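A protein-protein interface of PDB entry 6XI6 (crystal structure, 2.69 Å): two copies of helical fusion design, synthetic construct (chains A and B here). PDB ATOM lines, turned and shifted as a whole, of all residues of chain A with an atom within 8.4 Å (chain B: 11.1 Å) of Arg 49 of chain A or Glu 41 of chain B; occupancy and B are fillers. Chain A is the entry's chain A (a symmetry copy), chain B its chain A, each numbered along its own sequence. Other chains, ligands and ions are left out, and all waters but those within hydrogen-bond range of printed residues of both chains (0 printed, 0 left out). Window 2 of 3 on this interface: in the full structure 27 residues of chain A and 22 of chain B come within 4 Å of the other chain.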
ATOM      1  N   LEU A  35      28.423 -21.764  -3.118  1.00  0.00           N
ATOM      2  CA  LEU A  35      27.590 -20.750  -3.755  1.00  0.00           C
ATOM      3  C   LEU A  35      26.698 -21.363  -4.828  1.00  0.00           C
ATOM      4  O   LEU A  35      25.521 -21.001  -4.946  1.00  0.00           O
ATOM      5  CB  LEU A  35      28.468 -19.648  -4.346  1.00  0.00           C
ATOM      6  CG  LEU A  35      27.751 -18.458  -4.985  1.00  0.00           C
ATOM      7  CD1 LEU A  35      26.876 -17.744  -3.967  1.00  0.00           C
ATOM      8  CD2 LEU A  35      28.756 -17.495  -5.598  1.00  0.00           C
ATOM      9  N   THR A  39      22.687 -21.179  -4.743  1.00  0.00           N
ATOM     10  CA  THR A  39      22.012 -20.514  -5.853  1.00  0.00           C
ATOM     11  C   THR A  39      20.977 -21.422  -6.505  1.00  0.00           C
ATOM     12  O   THR A  39      19.948 -20.939  -6.994  1.00  0.00           O
ATOM     13  CB  THR A  39      23.040 -20.046  -6.887  1.00  0.00           C
ATOM     14  OG1 THR A  39      24.040 -19.249  -6.240  1.00  0.00           O
ATOM     15  CG2 THR A  39      22.374 -19.215  -7.976  1.00  0.00           C
ATOM     16  N   LEU A  42      17.885 -21.968  -3.366  1.00  0.00           N
ATOM     17  CA  LEU A  42      17.101 -20.819  -2.938  1.00  0.00           C
ATOM     18  C   LEU A  42      16.377 -20.180  -4.117  1.00  0.00           C
ATOM     19  O   LEU A  42      16.836 -20.233  -5.262  1.00  0.00           O
ATOM     20  CB  LEU A  42      17.995 -19.782  -2.256  1.00  0.00           C
ATOM     21  CG  LEU A  42      18.816 -20.272  -1.062  1.00  0.00           C
ATOM     22  CD1 LEU A  42      19.552 -19.115  -0.405  1.00  0.00           C
ATOM     23  CD2 LEU A  42      17.935 -20.995  -0.056  1.00  0.00           C
ATOM     24  N   ASP A  44      14.641 -16.889  -3.391  1.00  0.00           N
ATOM     25  CA  ASP A  44      14.589 -15.459  -3.116  1.00  0.00           C
ATOM     26  C   ASP A  44      15.788 -14.768  -3.751  1.00  0.00           C
ATOM     27  O   ASP A  44      16.938 -15.070  -3.413  1.00  0.00           O
ATOM     28  CB  ASP A  44      14.557 -15.212  -1.610  1.00  0.00           C
ATOM     29  CG  ASP A  44      14.467 -13.737  -1.263  1.00  0.00           C
ATOM     30  OD1 ASP A  44      13.450 -13.103  -1.613  1.00  0.00           O
ATOM     31  OD2 ASP A  44      15.413 -13.214  -0.637  1.00  0.00           O
ATOM     32  N   GLU A  45      15.521 -13.841  -4.674  1.00  0.00           N
ATOM     33  CA  GLU A  45      16.603 -13.126  -5.343  1.00  0.00           C
ATOM     34  C   GLU A  45      17.410 -12.282  -4.366  1.00  0.00           C
ATOM     35  O   GLU A  45      18.622 -12.123  -4.541  1.00  0.00           O
ATOM     36  CB  GLU A  45      16.044 -12.247  -6.462  1.00  0.00           C
ATOM     37  CG  GLU A  45      15.848 -12.954  -7.797  1.00  0.00           C
ATOM     38  CD  GLU A  45      14.941 -14.165  -7.702  1.00  0.00           C
ATOM     39  OE1 GLU A  45      15.462 -15.285  -7.517  1.00  0.00           O
ATOM     40  OE2 GLU A  45      13.706 -13.996  -7.806  1.00  0.00           O
ATOM     41  N   LYS A  46      16.759 -11.736  -3.335  1.00  0.00           N
ATOM     42  CA  LYS A  46      17.467 -10.901  -2.369  1.00  0.00           C
ATOM     43  C   LYS A  46      18.516 -11.703  -1.608  1.00  0.00           C
ATOM     44  O   LYS A  46      19.638 -11.228  -1.397  1.00  0.00           O
ATOM     45  CB  LYS A  46      16.471 -10.266  -1.400  1.00  0.00           C
ATOM     46  CG  LYS A  46      17.094  -9.299  -0.407  1.00  0.00           C
ATOM     47  CD  LYS A  46      17.695  -8.094  -1.114  1.00  0.00           C
ATOM     48  CE  LYS A  46      18.275  -7.103  -0.119  1.00  0.00           C
ATOM     49  NZ  LYS A  46      18.853  -5.911  -0.797  1.00  0.00           N
ATOM     50  N   THR A  47      18.171 -12.923  -1.192  1.00  0.00           N
ATOM     51  CA  THR A  47      19.123 -13.745  -0.451  1.00  0.00           C
ATOM     52  C   THR A  47      20.234 -14.257  -1.360  1.00  0.00           C
ATOM     53  O   THR A  47      21.392 -14.355  -0.937  1.00  0.00           O
ATOM     54  CB  THR A  47      18.396 -14.911   0.222  1.00  0.00           C
ATOM     55  OG1 THR A  47      17.314 -14.406   1.016  1.00  0.00           O
ATOM     56  CG2 THR A  47      19.348 -15.693   1.116  1.00  0.00           C
ATOM     57  N   ILE A  48      19.904 -14.580  -2.613  1.00  0.00           N
ATOM     58  CA  ILE A  48      20.908 -15.087  -3.545  1.00  0.00           C
ATOM     59  C   ILE A  48      21.973 -14.030  -3.812  1.00  0.00           C
ATOM     60  O   ILE A  48      23.173 -14.329  -3.839  1.00  0.00           O
ATOM     61  CB  ILE A  48      20.236 -15.560  -4.848  1.00  0.00           C
ATOM     62  CG1 ILE A  48      19.383 -16.802  -4.587  1.00  0.00           C
ATOM     63  CG2 ILE A  48      21.275 -15.839  -5.922  1.00  0.00           C
ATOM     64  CD1 ILE A  48      18.600 -17.272  -5.794  1.00  0.00           C
ATOM     65  N   ARG A  49      21.554 -12.776  -4.003  1.00  0.00           N
ATOM     66  CA  ARG A  49      22.510 -11.709  -4.283  1.00  0.00           C
ATOM     67  C   ARG A  49      23.429 -11.458  -3.093  1.00  0.00           C
ATOM     68  O   ARG A  49      24.620 -11.179  -3.271  1.00  0.00           O
ATOM     69  CB  ARG A  49      21.770 -10.430  -4.665  1.00  0.00           C
ATOM     70  CG  ARG A  49      21.018 -10.522  -5.979  1.00  0.00           C
ATOM     71  CD  ARG A  49      19.870  -9.532  -6.014  1.00  0.00           C
ATOM     72  NE  ARG A  49      19.062  -9.676  -7.221  1.00  0.00           N
ATOM     73  CZ  ARG A  49      17.825  -9.209  -7.348  1.00  0.00           C
ATOM     74  NH1 ARG A  49      17.162  -9.382  -8.482  1.00  0.00           N
ATOM     75  NH2 ARG A  49      17.248  -8.575  -6.336  1.00  0.00           N
ATOM     76  N   GLU A  50      22.896 -11.548  -1.872  1.00  0.00           N
ATOM     77  CA  GLU A  50      23.731 -11.336  -0.696  1.00  0.00           C
ATOM     78  C   GLU A  50      24.699 -12.492  -0.480  1.00  0.00           C
ATOM     79  O   GLU A  50      25.821 -12.279  -0.008  1.00  0.00           O
ATOM     80  CB  GLU A  50      22.857 -11.128   0.542  1.00  0.00           C
ATOM     81  CG  GLU A  50      21.921  -9.932   0.444  1.00  0.00           C
ATOM     82  CD  GLU A  50      22.657  -8.622   0.221  1.00  0.00           C
ATOM     83  OE1 GLU A  50      23.791  -8.476   0.724  1.00  0.00           O
ATOM     84  OE2 GLU A  50      22.099  -7.735  -0.461  1.00  0.00           O
ATOM     85  N   GLU A  51      24.287 -13.717  -0.818  1.00  0.00           N
ATOM     86  CA  GLU A  51      25.215 -14.842  -0.766  1.00  0.00           C
ATOM     87  C   GLU A  51      26.331 -14.685  -1.789  1.00  0.00           C
ATOM     88  O   GLU A  51      27.454 -15.146  -1.556  1.00  0.00           O
ATOM     89  CB  GLU A  51      24.468 -16.157  -0.997  1.00  0.00           C
ATOM     90  CG  GLU A  51      23.468 -16.520   0.092  1.00  0.00           C
ATOM     91  CD  GLU A  51      24.133 -16.983   1.375  1.00  0.00           C
ATOM     92  OE1 GLU A  51      25.354 -17.247   1.359  1.00  0.00           O
ATOM     93  OE2 GLU A  51      23.428 -17.089   2.402  1.00  0.00           O
ATOM     94  N   ILE A  52      26.048 -14.037  -2.920  1.00  0.00           N
ATOM     95  CA  ILE A  52      27.070 -13.837  -3.941  1.00  0.00           C
ATOM     96  C   ILE A  52      28.051 -12.754  -3.511  1.00  0.00           C
ATOM     97  O   ILE A  52      29.267 -12.890  -3.696  1.00  0.00           O
ATOM     98  CB  ILE A  52      26.413 -13.505  -5.293  1.00  0.00           C
ATOM     99  CG1 ILE A  52      25.639 -14.714  -5.824  1.00  0.00           C
ATOM    100  CG2 ILE A  52      27.458 -13.053  -6.305  1.00  0.00           C
ATOM    101  CD1 ILE A  52      24.876 -14.436  -7.100  1.00  0.00           C
ATOM    102  N   ARG A  53      27.546 -11.668  -2.921  1.00  0.00           N
ATOM    103  CA  ARG A  53      28.418 -10.556  -2.558  1.00  0.00           C
ATOM    104  C   ARG A  53      29.360 -10.934  -1.421  1.00  0.00           C
ATOM    105  O   ARG A  53      30.522 -10.511  -1.406  1.00  0.00           O
ATOM    106  CB  ARG A  53      27.587  -9.333  -2.175  1.00  0.00           C
ATOM    107  CG  ARG A  53      28.339  -8.016  -2.311  1.00  0.00           C
ATOM    108  CD  ARG A  53      27.900  -7.000  -1.267  1.00  0.00           C
ATOM    109  NE  ARG A  53      28.455  -7.296   0.051  1.00  0.00           N
ATOM    110  CZ  ARG A  53      27.800  -7.935   1.015  1.00  0.00           C
ATOM    111  NH1 ARG A  53      26.555  -8.346   0.816  1.00  0.00           N
ATOM    112  NH2 ARG A  53      28.388  -8.160   2.181  1.00  0.00           N
ATOM    113  N   LYS A  54      28.881 -11.727  -0.457  1.00  0.00           N
ATOM    114  CA  LYS A  54      29.747 -12.141   0.641  1.00  0.00           C
ATOM    115  C   LYS A  54      30.828 -13.104   0.165  1.00  0.00           C
ATOM    116  O   LYS A  54      31.909 -13.161   0.759  1.00  0.00           O
ATOM    117  CB  LYS A  54      28.925 -12.774   1.764  1.00  0.00           C
ATOM    118  CG  LYS A  54      28.310 -14.119   1.417  1.00  0.00           C
ATOM    119  CD  LYS A  54      27.748 -14.808   2.651  1.00  0.00           C
ATOM    120  CE  LYS A  54      26.651 -13.981   3.300  1.00  0.00           C
ATOM    121  NZ  LYS A  54      26.080 -14.660   4.497  1.00  0.00           N
ATOM    122  N   VAL A  55      30.556 -13.864  -0.898  1.00  0.00           N
ATOM    123  CA  VAL A  55      31.583 -14.727  -1.471  1.00  0.00           C
ATOM    124  C   VAL A  55      32.592 -13.905  -2.260  1.00  0.00           C
ATOM    125  O   VAL A  55      33.800 -14.157  -2.195  1.00  0.00           O
ATOM    126  CB  VAL A  55      30.933 -15.823  -2.337  1.00  0.00           C
ATOM    127  CG1 VAL A  55      31.984 -16.546  -3.166  1.00  0.00           C
ATOM    128  CG2 VAL A  55      30.182 -16.812  -1.461  1.00  0.00           C
ATOM    129  N   LYS A  56      32.120 -12.902  -3.005  1.00  0.00           N
ATOM    130  CA  LYS A  56      33.034 -12.030  -3.732  1.00  0.00           C
ATOM    131  C   LYS A  56      33.891 -11.204  -2.781  1.00  0.00           C
ATOM    132  O   LYS A  56      35.060 -10.931  -3.079  1.00  0.00           O
ATOM    133  CB  LYS A  56      32.251 -11.119  -4.678  1.00  0.00           C
ATOM    134  CG  LYS A  56      33.125 -10.315  -5.627  1.00  0.00           C
ATOM    135  CD  LYS A  56      32.295  -9.587  -6.671  1.00  0.00           C
ATOM    136  CE  LYS A  56      33.182  -8.892  -7.691  1.00  0.00           C
ATOM    137  NZ  LYS A  56      32.388  -8.226  -8.761  1.00  0.00           N
ATOM    138  N   ASN B  32      34.388 -16.784 -12.255  1.00  0.00           N
ATOM    139  CA  ASN B  32      33.391 -17.687 -11.688  1.00  0.00           C
ATOM    140  C   ASN B  32      32.286 -16.914 -10.979  1.00  0.00           C
ATOM    141  O   ASN B  32      31.097 -17.203 -11.160  1.00  0.00           O
ATOM    142  CB  ASN B  32      34.058 -18.674 -10.728  1.00  0.00           C
ATOM    143  CG  ASN B  32      35.084 -19.553 -11.413  1.00  0.00           C
ATOM    144  OD1 ASN B  32      35.034 -19.757 -12.625  1.00  0.00           O
ATOM    145  ND2 ASN B  32      36.023 -20.083 -10.636  1.00  0.00           N
ATOM    146  N   ILE B  33      32.661 -15.922 -10.169  1.00  0.00           N
ATOM    147  CA  ILE B  33      31.666 -15.157  -9.423  1.00  0.00           C
ATOM    148  C   ILE B  33      30.810 -14.324 -10.370  1.00  0.00           C
ATOM    149  O   ILE B  33      29.596 -14.192 -10.175  1.00  0.00           O
ATOM    150  CB  ILE B  33      32.354 -14.284  -8.358  1.00  0.00           C
ATOM    151  CG1 ILE B  33      33.259 -15.141  -7.471  1.00  0.00           C
ATOM    152  CG2 ILE B  33      31.320 -13.558  -7.511  1.00  0.00           C
ATOM    153  CD1 ILE B  33      32.547 -16.301  -6.809  1.00  0.00           C
ATOM    154  N   ASP B  34      31.425 -13.754 -11.409  1.00  0.00           N
ATOM    155  CA  ASP B  34      30.656 -12.999 -12.394  1.00  0.00           C
ATOM    156  C   ASP B  34      29.713 -13.902 -13.176  1.00  0.00           C
ATOM    157  O   ASP B  34      28.609 -13.479 -13.539  1.00  0.00           O
ATOM    158  CB  ASP B  34      31.597 -12.263 -13.349  1.00  0.00           C
ATOM    159  CG  ASP B  34      32.378 -11.156 -12.665  1.00  0.00           C
ATOM    160  OD1 ASP B  34      32.141 -10.914 -11.463  1.00  0.00           O
ATOM    161  OD2 ASP B  34      33.230 -10.530 -13.329  1.00  0.00           O
ATOM    162  N   LEU B  35      30.123 -15.145 -13.440  1.00  0.00           N
ATOM    163  CA  LEU B  35      29.272 -16.063 -14.188  1.00  0.00           C
ATOM    164  C   LEU B  35      28.089 -16.530 -13.348  1.00  0.00           C
ATOM    165  O   LEU B  35      26.963 -16.626 -13.850  1.00  0.00           O
ATOM    166  CB  LEU B  35      30.093 -17.255 -14.678  1.00  0.00           C
ATOM    167  CG  LEU B  35      29.371 -18.281 -15.554  1.00  0.00           C
ATOM    168  CD1 LEU B  35      28.845 -17.632 -16.824  1.00  0.00           C
ATOM    169  CD2 LEU B  35      30.294 -19.442 -15.886  1.00  0.00           C
ATOM    170  N   VAL B  36      28.326 -16.826 -12.066  1.00  0.00           N
ATOM    171  CA  VAL B  36      27.239 -17.233 -11.180  1.00  0.00           C
ATOM    172  C   VAL B  36      26.232 -16.099 -11.020  1.00  0.00           C
ATOM    173  O   VAL B  36      25.021 -16.333 -10.920  1.00  0.00           O
ATOM    174  CB  VAL B  36      27.802 -17.692  -9.820  1.00  0.00           C
ATOM    175  CG1 VAL B  36      26.676 -17.950  -8.826  1.00  0.00           C
ATOM    176  CG2 VAL B  36      28.648 -18.943  -9.995  1.00  0.00           C
ATOM    177  N   ARG B  37      26.715 -14.855 -11.006  1.00  0.00           N
ATOM    178  CA  ARG B  37      25.817 -13.710 -10.892  1.00  0.00           C
ATOM    179  C   ARG B  37      24.941 -13.572 -12.132  1.00  0.00           C
ATOM    180  O   ARG B  37      23.726 -13.366 -12.026  1.00  0.00           O
ATOM    181  CB  ARG B  37      26.623 -12.432 -10.658  1.00  0.00           C
ATOM    182  CG  ARG B  37      25.801 -11.163 -10.765  1.00  0.00           C
ATOM    183  CD  ARG B  37      26.682  -9.926 -10.800  1.00  0.00           C
ATOM    184  NE  ARG B  37      25.949  -8.762 -11.285  1.00  0.00           N
ATOM    185  CZ  ARG B  37      25.832  -8.438 -12.569  1.00  0.00           C
ATOM    186  NH1 ARG B  37      25.145  -7.361 -12.924  1.00  0.00           N
ATOM    187  NH2 ARG B  37      26.402  -9.192 -13.499  1.00  0.00           N
ATOM    188  N   LYS B  38      25.542 -13.683 -13.320  1.00  0.00           N
ATOM    189  CA  LYS B  38      24.774 -13.527 -14.551  1.00  0.00           C
ATOM    190  C   LYS B  38      23.852 -14.716 -14.800  1.00  0.00           C
ATOM    191  O   LYS B  38      22.769 -14.548 -15.372  1.00  0.00           O
ATOM    192  CB  LYS B  38      25.717 -13.327 -15.735  1.00  0.00           C
ATOM    193  CG  LYS B  38      26.506 -12.029 -15.678  1.00  0.00           C
ATOM    194  CD  LYS B  38      27.487 -11.917 -16.836  1.00  0.00           C
ATOM    195  CE  LYS B  38      28.298 -10.633 -16.745  1.00  0.00           C
ATOM    196  NZ  LYS B  38      29.307 -10.532 -17.836  1.00  0.00           N
ATOM    197  N   THR B  39      24.258 -15.917 -14.382  1.00  0.00           N
ATOM    198  CA  THR B  39      23.410 -17.088 -14.577  1.00  0.00           C
ATOM    199  C   THR B  39      22.159 -17.027 -13.709  1.00  0.00           C
ATOM    200  O   THR B  39      21.099 -17.523 -14.111  1.00  0.00           O
ATOM    201  CB  THR B  39      24.203 -18.365 -14.285  1.00  0.00           C
ATOM    202  OG1 THR B  39      25.406 -18.369 -15.063  1.00  0.00           O
ATOM    203  CG2 THR B  39      23.385 -19.602 -14.631  1.00  0.00           C
ATOM    204  N   SER B  40      22.252 -16.413 -12.528  1.00  0.00           N
ATOM    205  CA  SER B  40      21.107 -16.350 -11.628  1.00  0.00           C
ATOM    206  C   SER B  40      20.151 -15.218 -11.983  1.00  0.00           C
ATOM    207  O   SER B  40      18.960 -15.298 -11.661  1.00  0.00           O
ATOM    208  CB  SER B  40      21.583 -16.195 -10.182  1.00  0.00           C
ATOM    209  OG  SER B  40      22.290 -14.979 -10.007  1.00  0.00           O
ATOM    210  N   GLU B  41      20.642 -14.167 -12.639  1.00  0.00           N
ATOM    211  CA  GLU B  41      19.805 -13.021 -12.974  1.00  0.00           C
ATOM    212  C   GLU B  41      19.121 -13.182 -14.328  1.00  0.00           C
ATOM    213  O   GLU B  41      17.917 -12.936 -14.452  1.00  0.00           O
ATOM    214  CB  GLU B  41      20.642 -11.736 -12.959  1.00  0.00           C
ATOM    215  CG  GLU B  41      21.245 -11.385 -11.604  1.00  0.00           C
ATOM    216  CD  GLU B  41      20.235 -10.800 -10.633  1.00  0.00           C
ATOM    217  OE1 GLU B  41      19.053 -10.649 -11.006  1.00  0.00           O
ATOM    218  OE2 GLU B  41      20.630 -10.482  -9.491  1.00  0.00           O
ATOM    219  N   LEU B  42      19.871 -13.593 -15.347  1.00  0.00           N
ATOM    220  CA  LEU B  42      19.336 -13.679 -16.697  1.00  0.00           C
ATOM    221  C   LEU B  42      18.421 -14.888 -16.849  1.00  0.00           C
ATOM    222  O   LEU B  42      18.584 -15.910 -16.175  1.00  0.00           O
ATOM    223  CB  LEU B  42      20.471 -13.757 -17.721  1.00  0.00           C
ATOM    224  CG  LEU B  42      21.498 -12.624 -17.684  1.00  0.00           C
ATOM    225  CD1 LEU B  42      22.487 -12.759 -18.832  1.00  0.00           C
ATOM    226  CD2 LEU B  42      20.814 -11.267 -17.715  1.00  0.00           C
ATOM    227  N   THR B  43      17.447 -14.760 -17.754  1.00  0.00           N
ATOM    228  CA  THR B  43      16.514 -15.836 -18.052  1.00  0.00           C
ATOM    229  C   THR B  43      16.643 -16.382 -19.465  1.00  0.00           C
ATOM    230  O   THR B  43      16.168 -17.492 -19.724  1.00  0.00           O
ATOM    231  CB  THR B  43      15.066 -15.371 -17.839  1.00  0.00           C
ATOM    232  OG1 THR B  43      14.771 -14.289 -18.731  1.00  0.00           O
ATOM    233  CG2 THR B  43      14.860 -14.909 -16.406  1.00  0.00           C
ATOM    234  N   ASP B  44      17.263 -15.640 -20.379  1.00  0.00           N
ATOM    235  CA  ASP B  44      17.428 -16.111 -21.748  1.00  0.00           C
ATOM    236  C   ASP B  44      18.505 -17.186 -21.797  1.00  0.00           C
ATOM    237  O   ASP B  44      19.665 -16.929 -21.455  1.00  0.00           O
ATOM    238  CB  ASP B  44      17.784 -14.948 -22.669  1.00  0.00           C
ATOM    239  CG  ASP B  44      17.934 -15.374 -24.117  1.00  0.00           C
ATOM    240  OD1 ASP B  44      16.934 -15.828 -24.712  1.00  0.00           O
ATOM    241  OD2 ASP B  44      19.052 -15.251 -24.662  1.00  0.00           O
ATOM    242  N   GLU B  45      18.122 -18.394 -22.220  1.00  0.00           N
ATOM    243  CA  GLU B  45      19.081 -19.491 -22.298  1.00  0.00           C
ATOM    244  C   GLU B  45      20.182 -19.208 -23.311  1.00  0.00           C
ATOM    245  O   GLU B  45      21.327 -19.628 -23.113  1.00  0.00           O
ATOM    246  CB  GLU B  45      18.364 -20.796 -22.649  1.00  0.00           C
ATOM    247  CG  GLU B  45      17.781 -21.550 -21.460  1.00  0.00           C
ATOM    248  CD  GLU B  45      16.803 -20.720 -20.652  1.00  0.00           C
ATOM    249  OE1 GLU B  45      17.233 -20.085 -19.666  1.00  0.00           O
ATOM    250  OE2 GLU B  45      15.604 -20.698 -21.006  1.00  0.00           O
ATOM    251  N   THR B  47      21.611 -16.304 -24.078  1.00  0.00           N
ATOM    252  CA  THR B  47      22.621 -15.412 -23.518  1.00  0.00           C
ATOM    253  C   THR B  47      23.423 -16.105 -22.423  1.00  0.00           C
ATOM    254  O   THR B  47      24.631 -15.879 -22.294  1.00  0.00           O
ATOM    255  CB  THR B  47      21.959 -14.143 -22.980  1.00  0.00           C
ATOM    256  OG1 THR B  47      21.158 -13.548 -24.009  1.00  0.00           O
ATOM    257  CG2 THR B  47      23.012 -13.139 -22.525  1.00  0.00           C
ATOM    258  N   ILE B  48      22.770 -16.960 -21.630  1.00  0.00           N
ATOM    259  CA  ILE B  48      23.463 -17.659 -20.551  1.00  0.00           C
ATOM    260  C   ILE B  48      24.537 -18.583 -21.114  1.00  0.00           C
ATOM    261  O   ILE B  48      25.657 -18.645 -20.594  1.00  0.00           O
ATOM    262  CB  ILE B  48      22.452 -18.427 -19.678  1.00  0.00           C
ATOM    263  CG1 ILE B  48      21.562 -17.450 -18.908  1.00  0.00           C
ATOM    264  CG2 ILE B  48      23.169 -19.366 -18.720  1.00  0.00           C
ATOM    265  CD1 ILE B  48      20.468 -18.119 -18.105  1.00  0.00           C
ATOM    266  N   GLU B  51      27.521 -16.552 -22.295  1.00  0.00           N
ATOM    267  CA  GLU B  51      28.312 -16.094 -21.158  1.00  0.00           C
ATOM    268  C   GLU B  51      29.160 -17.219 -20.583  1.00  0.00           C
ATOM    269  O   GLU B  51      30.252 -16.966 -20.061  1.00  0.00           O
ATOM    270  CB  GLU B  51      27.398 -15.516 -20.074  1.00  0.00           C
ATOM    271  CG  GLU B  51      26.657 -14.249 -20.478  1.00  0.00           C
ATOM    272  CD  GLU B  51      27.557 -13.029 -20.538  1.00  0.00           C
ATOM    273  OE1 GLU B  51      28.705 -13.104 -20.050  1.00  0.00           O
ATOM    274  OE2 GLU B  51      27.113 -11.991 -21.073  1.00  0.00           O
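The side-chain carboxylate (OE2) of Glu 41 of chain B is in salt-bridge range of the guanidinium group (NE) of Arg 49 of chain A (2.9 Å).
The side-chain amino group (NZ) of Lys 56 of chain A lies within salt-bridge range of the side-chain carboxylate (OD1) of Asp 34 of chain B, at 3.8 Å.
The backbone carbonyl oxygen (O) of Leu 35 of chain A is in hydrogen-bond range of the side-chain hydroxyl (OG1) of Thr 39 of chain A, at 2.6 Å.
O of Arg 37 of chain B is in hydrogen-bond range of OG of Ser 40 of chain B, 3.0 Å away.
O of Val 36 of chain B is in hydrogen-bond range of OG of Ser 40 of chain B (3.2 Å).
Val 36 of chain B touches Leu 35 of chain A (CG1 to CD2, 3.9 Å).
Val 36 of chain B touches Thr 39 of chain A (CG1 to OG1, 3.9 Å).
Thr 39 of chain A touches Ser 40 of chain B (CG2 to CB, 3.8 Å).
Ile 52 of chain A touches Arg 37 of chain B (CD1 to CA, 3.97 Å).
Ile 52 of chain A touches Ser 40 of chain B (CD1 to OG, 3.9 Å).
CD1 of Ile 33 of chain B touches CG1 of Val 55 of chain A, at 3.7 Å.
Lys 56 of chain A touches Ile 33 of chain B (CB to CG2, 3.9 Å).
8 positions are printed for both chains.
Of the 9 pairs that touch across the chains among the printed residues, none has its exchanged pair printed and touching as well.
Of the 16 printed residues of chain A, 6 touch a printed residue of chain B.
Hydrophobic or aromatic side chains of chain A that line the printed part of chain B: Leu 35, Ile 52 and Val 55.
Among the printed residues, 9 pairs touch across the chains.
Among the printed residues, Asp or Glu carboxylates within 4 Å of a Lys or Arg side-chain nitrogen of the other chain: Arg 49 of chain A with Glu 41 of chain B and Lys 56 of chain A with Asp 34 of chain B.
Arg 49 of chain A touches just one residue of chain B: Glu 41 (2.9 Å).
Glu 41 of chain B touches just one residue of chain A: Arg 49.
No residue of chain B comes within 4 Å of Glu 45 of chain A.
No residue of chain B comes within 4 Å of Lys 46 of chain A.
No residue of chain B comes within 4 Å of Glu 50 of chain A.
Of the printed residues of chain B, Ile 52 of chain A touches Arg 37 (3.97 Å) and Ser 40 (3.9 Å).
Of the printed residues of chain A, Ser 40 of chain B touches Thr 39 and Ile 52.
Printed residues of chain B within 4 Å of Leu 35 of chain A: Val 36.
Printed residues of chain B within 4 Å of Thr 39 of chain A: Val 36 and Ser 40.
Leu 42 of chain B touches none of the printed residues of chain A.
Lys 38 of chain B touches none of the printed residues of chain A.
The nearest residue of chain B that does not touch Arg 49 of chain A is Ser 40 of chain B (6.1 Å).
The nearest residue of chain A that does not touch Glu 41 of chain B is Glu 45 of chain A (5.1 Å).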
